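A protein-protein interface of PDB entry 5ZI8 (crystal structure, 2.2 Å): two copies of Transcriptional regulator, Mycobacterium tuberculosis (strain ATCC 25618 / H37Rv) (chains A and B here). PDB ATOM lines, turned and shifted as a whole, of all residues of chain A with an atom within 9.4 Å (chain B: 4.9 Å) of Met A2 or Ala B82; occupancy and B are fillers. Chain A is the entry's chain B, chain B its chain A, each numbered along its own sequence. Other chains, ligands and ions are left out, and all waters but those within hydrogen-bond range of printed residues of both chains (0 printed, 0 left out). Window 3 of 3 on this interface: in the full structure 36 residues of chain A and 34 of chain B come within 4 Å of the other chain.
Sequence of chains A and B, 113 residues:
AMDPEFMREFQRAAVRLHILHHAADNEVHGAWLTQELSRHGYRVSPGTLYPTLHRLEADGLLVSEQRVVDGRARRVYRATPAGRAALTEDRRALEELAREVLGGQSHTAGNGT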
ATOM      1  N   ALA A   1     -26.800   3.340  13.777  1.00  0.00           N
ATOM      2  CA  ALA A   1     -27.070   2.319  12.712  1.00  0.00           C
ATOM      3  C   ALA A   1     -27.860   2.974  11.555  1.00  0.00           C
ATOM      4  O   ALA A   1     -29.012   3.501  11.724  1.00  0.00           O
ATOM      5  CB  ALA A   1     -27.833   1.150  13.296  1.00  0.00           C
ATOM      6  N   MET A   2     -27.244   2.994  10.385  1.00  0.00           N
ATOM      7  CA  MET A   2     -27.939   3.574   9.251  1.00  0.00           C
ATOM      8  C   MET A   2     -29.140   2.740   8.849  1.00  0.00           C
ATOM      9  O   MET A   2     -30.157   3.281   8.367  1.00  0.00           O
ATOM     10  CB  MET A   2     -26.982   3.767   8.097  1.00  0.00           C
ATOM     11  CG  MET A   2     -25.894   4.778   8.378  1.00  0.00           C
ATOM     12  SD  MET A   2     -26.606   6.411   8.593  1.00  0.00           S
ATOM     13  CE  MET A   2     -27.326   6.725   6.984  1.00  0.00           C
ATOM     14  N   ASP A   3     -29.055   1.430   9.086  1.00  0.00           N
ATOM     15  CA  ASP A   3     -30.073   0.486   8.673  1.00  0.00           C
ATOM     16  C   ASP A   3     -30.425  -0.419   9.851  1.00  0.00           C
ATOM     17  O   ASP A   3     -29.933  -1.543   9.976  1.00  0.00           O
ATOM     18  CB  ASP A   3     -29.553  -0.280   7.475  1.00  0.00           C
ATOM     19  CG  ASP A   3     -30.613  -1.076   6.762  1.00  0.00           C
ATOM     20  OD1 ASP A   3     -31.808  -1.124   7.232  1.00  0.00           O
ATOM     21  OD2 ASP A   3     -30.201  -1.678   5.733  1.00  0.00           O
ATOM     22  N   PRO A   4     -31.303   0.093  10.727  1.00  0.00           N
ATOM     23  CA  PRO A   4     -31.679  -0.641  11.908  1.00  0.00           C
ATOM     24  C   PRO A   4     -32.469  -1.866  11.610  1.00  0.00           C
ATOM     25  O   PRO A   4     -32.337  -2.826  12.345  1.00  0.00           O
ATOM     26  CB  PRO A   4     -32.502   0.355  12.720  1.00  0.00           C
ATOM     27  CG  PRO A   4     -32.239   1.672  12.115  1.00  0.00           C
ATOM     28  CD  PRO A   4     -31.963   1.407  10.680  1.00  0.00           C
ATOM     29  N   GLU A   5     -33.256  -1.867  10.555  1.00  0.00           N
ATOM     30  CA  GLU A   5     -34.031  -3.044  10.208  1.00  0.00           C
ATOM     31  C   GLU A   5     -33.151  -4.181   9.762  1.00  0.00           C
ATOM     32  O   GLU A   5     -33.347  -5.314  10.172  1.00  0.00           O
ATOM     33  CB  GLU A   5     -35.079  -2.720   9.105  1.00  0.00           C
ATOM     34  CG  GLU A   5     -35.911  -3.929   8.637  1.00  0.00           C
ATOM     35  CD  GLU A   5     -36.617  -4.691   9.797  1.00  0.00           C
ATOM     36  OE1 GLU A   5     -36.889  -4.069  10.845  1.00  0.00           O
ATOM     37  OE2 GLU A   5     -36.951  -5.904   9.698  1.00  0.00           O
ATOM     38  N   PHE A   6     -32.202  -3.876   8.887  1.00  0.00           N
ATOM     39  CA  PHE A   6     -31.202  -4.838   8.512  1.00  0.00           C
ATOM     40  C   PHE A   6     -30.488  -5.400   9.724  1.00  0.00           C
ATOM     41  O   PHE A   6     -30.328  -6.587   9.823  1.00  0.00           O
ATOM     42  CB  PHE A   6     -30.142  -4.253   7.617  1.00  0.00           C
ATOM     43  CG  PHE A   6     -29.064  -5.241   7.307  1.00  0.00           C
ATOM     44  CD1 PHE A   6     -29.252  -6.194   6.288  1.00  0.00           C
ATOM     45  CD2 PHE A   6     -27.913  -5.305   8.072  1.00  0.00           C
ATOM     46  CE1 PHE A   6     -28.272  -7.127   6.007  1.00  0.00           C
ATOM     47  CE2 PHE A   6     -26.954  -6.247   7.812  1.00  0.00           C
ATOM     48  CZ  PHE A   6     -27.123  -7.160   6.790  1.00  0.00           C
ATOM     49  N   MET A   7     -30.030  -4.533  10.609  1.00  0.00           N
ATOM     50  CA  MET A   7     -29.281  -4.994  11.795  1.00  0.00           C
ATOM     51  C   MET A   7     -30.073  -5.910  12.679  1.00  0.00           C
ATOM     52  O   MET A   7     -29.596  -6.938  13.116  1.00  0.00           O
ATOM     53  CB  MET A   7     -28.737  -3.824  12.617  1.00  0.00           C
ATOM     54  CG  MET A   7     -27.625  -3.094  11.888  1.00  0.00           C
ATOM     55  SD  MET A   7     -26.178  -4.120  11.425  1.00  0.00           S
ATOM     56  CE  MET A   7     -25.425  -2.961  10.273  1.00  0.00           C
ATOM     57  N   GLY B  60     -35.435   6.318   4.332  1.00  0.00           N
ATOM     58  CA  GLY B  60     -34.527   7.246   3.693  1.00  0.00           C
ATOM     59  C   GLY B  60     -33.359   6.573   2.943  1.00  0.00           C
ATOM     60  O   GLY B  60     -32.404   7.261   2.517  1.00  0.00           O
ATOM     61  N   LEU B  61     -33.390   5.256   2.763  1.00  0.00           N
ATOM     62  CA  LEU B  61     -32.246   4.593   2.184  1.00  0.00           C
ATOM     63  C   LEU B  61     -32.392   4.482   0.686  1.00  0.00           C
ATOM     64  O   LEU B  61     -31.393   4.334  -0.034  1.00  0.00           O
ATOM     65  CB  LEU B  61     -31.997   3.208   2.831  1.00  0.00           C
ATOM     66  CG  LEU B  61     -31.867   3.241   4.374  1.00  0.00           C
ATOM     67  CD1 LEU B  61     -31.672   1.882   4.987  1.00  0.00           C
ATOM     68  CD2 LEU B  61     -30.810   4.202   4.882  1.00  0.00           C
ATOM     69  N   THR B  80     -29.931   6.544  -1.865  1.00  0.00           N
ATOM     70  CA  THR B  80     -29.598   7.879  -1.414  1.00  0.00           C
ATOM     71  C   THR B  80     -28.223   7.788  -0.806  1.00  0.00           C
ATOM     72  O   THR B  80     -27.700   6.692  -0.594  1.00  0.00           O
ATOM     73  CB  THR B  80     -30.556   8.272  -0.302  1.00  0.00           C
ATOM     74  OG1 THR B  80     -30.441   7.305   0.755  1.00  0.00           O
ATOM     75  CG2 THR B  80     -32.028   8.247  -0.851  1.00  0.00           C
ATOM     76  N   PRO B  81     -27.614   8.933  -0.484  1.00  0.00           N
ATOM     77  CA  PRO B  81     -26.391   8.889   0.264  1.00  0.00           C
ATOM     78  C   PRO B  81     -26.462   8.036   1.532  1.00  0.00           C
ATOM     79  O   PRO B  81     -25.513   7.287   1.862  1.00  0.00           O
ATOM     80  CB  PRO B  81     -26.161  10.350   0.595  1.00  0.00           C
ATOM     81  CG  PRO B  81     -26.638  11.041  -0.670  1.00  0.00           C
ATOM     82  CD  PRO B  81     -27.912  10.294  -0.951  1.00  0.00           C
ATOM     83  N   ALA B  82     -27.568   8.131   2.237  1.00  0.00           N
ATOM     84  CA  ALA B  82     -27.739   7.361   3.458  1.00  0.00           C
ATOM     85  C   ALA B  82     -27.793   5.867   3.127  1.00  0.00           C
ATOM     86  O   ALA B  82     -27.283   5.053   3.876  1.00  0.00           O
ATOM     87  CB  ALA B  82     -29.030   7.789   4.167  1.00  0.00           C
ATOM     88  N   GLY B  83     -28.421   5.517   2.006  1.00  0.00           N
ATOM     89  CA  GLY B  83     -28.448   4.168   1.556  1.00  0.00           C
ATOM     90  C   GLY B  83     -27.072   3.588   1.264  1.00  0.00           C
ATOM     91  O   GLY B  83     -26.801   2.411   1.564  1.00  0.00           O
ATOM     92  N   ARG B  84     -26.193   4.396   0.665  1.00  0.00           N
ATOM     93  CA  ARG B  84     -24.816   3.929   0.410  1.00  0.00           C
ATOM     94  C   ARG B  84     -24.076   3.693   1.715  1.00  0.00           C
ATOM     95  O   ARG B  84     -23.361   2.714   1.873  1.00  0.00           O
ATOM     96  CB  ARG B  84     -24.047   4.917  -0.421  1.00  0.00           C
ATOM     97  CG  ARG B  84     -24.549   4.970  -1.845  1.00  0.00           C
ATOM     98  CD  ARG B  84     -23.697   5.873  -2.752  1.00  0.00           C
ATOM     99  NE  ARG B  84     -24.190   5.653  -4.110  1.00  0.00           N
ATOM    100  CZ  ARG B  84     -25.288   6.222  -4.616  1.00  0.00           C
ATOM    101  NH1 ARG B  84     -25.976   7.127  -3.881  1.00  0.00           N
ATOM    102  NH2 ARG B  84     -25.691   5.921  -5.867  1.00  0.00           N
ATOM    103  N   ALA B  85     -24.255   4.615   2.649  1.00  0.00           N
ATOM    104  CA  ALA B  85     -23.646   4.469   3.956  1.00  0.00           C
ATOM    105  C   ALA B  85     -24.190   3.205   4.616  1.00  0.00           C
ATOM    106  O   ALA B  85     -23.434   2.460   5.170  1.00  0.00           O
ATOM    107  CB  ALA B  85     -23.934   5.698   4.813  1.00  0.00           C
ATOM    108  N   ALA B  86     -25.504   2.970   4.531  1.00  0.00           N
ATOM    109  CA  ALA B  86     -26.114   1.771   5.106  1.00  0.00           C
ATOM    110  C   ALA B  86     -25.547   0.492   4.506  1.00  0.00           C
ATOM    111  O   ALA B  86     -25.295  -0.485   5.205  1.00  0.00           O
ATOM    112  CB  ALA B  86     -27.617   1.791   4.931  1.00  0.00           C
ATOM    113  N   GLU B  89     -22.282  -0.276   6.044  1.00  0.00           N
ATOM    114  CA  GLU B  89     -22.424  -0.737   7.416  1.00  0.00           C
ATOM    115  C   GLU B  89     -22.947  -2.184   7.423  1.00  0.00           C
ATOM    116  O   GLU B  89     -22.468  -3.007   8.205  1.00  0.00           O
ATOM    117  CB  GLU B  89     -23.339   0.179   8.229  1.00  0.00           C
ATOM    118  CG  GLU B  89     -22.752   1.551   8.540  1.00  0.00           C
ATOM    119  CD  GLU B  89     -23.572   2.396   9.568  1.00  0.00           C
ATOM    120  OE1 GLU B  89     -24.618   1.921  10.114  1.00  0.00           O
ATOM    121  OE2 GLU B  89     -23.169   3.564   9.838  1.00  0.00           O
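OD1 of Asp A3 is in hydrogen-bond range of N of Phe A6 (3.2 Å). The backbone NH of Ala B82 sits close to the side-chain hydroxyl of Thr B80. The side-chain hydroxyl (OG1) of Thr B80 is in hydrogen-bond range of the backbone carbonyl oxygen (O) of Leu B61, at 3.2 Å.
The side-chain carboxylate (OE1) of Glu B89 sits at hydrogen-bond distance from the backbone NH (N) of Met A2, at 2.8 Å.
Hydrophobic or aromatic side chains of chain A that line the printed part of chain B: Met A2 and Met A7. Along chain A the printed residues that touch a printed residue of chain B span positions 1 to 7. Printed residues of chain B that touch a printed residue of chain A: Leu B61, Ala B82, Ala B86 and Glu B89.
Of the printed residues of chain B, Ala A1 touches Glu B89. Met A2 touches four residues of chain B. Printed residues of chain B within 4 Å of Asp A3: Leu B61 (3.6 Å) and Ala B86 (3.8 Å). Printed residues of chain B within 4 Å of Met A7: Glu B89. Printed residues of chain A within 4 Å of Leu B61: Met A2 and Asp A3. Thr B80 touches none of the printed residues of chain A. No residue of chain A comes within 4 Å of Pro B81. Printed residues of chain A within 4 Å of Ala B82: Met A2 (3.5 Å). No residue of chain A comes within 4 Å of Gly B83. Arg B84 touches none of the printed residues of chain A. No residue of chain A comes within 4 Å of Ala B85. The nearest residue of chain A that does not touch Ala B82 is Asp A3 (6.6 Å).
No position is printed for both chains.
Among the printed residues, merely in contact across the chains: Ala A1 with Glu B89 (3.6 Å), Met A2 with Leu B61 (3.7 Å), Met A2 with Ala B82 (3.5 Å), Met A2 with Ala B86 (3.7 Å), Asp A3 with Leu B61 (3.6 Å), Asp A3 with Ala B86 (3.8 Å) and Met A7 with Glu B89 (3.6 Å).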
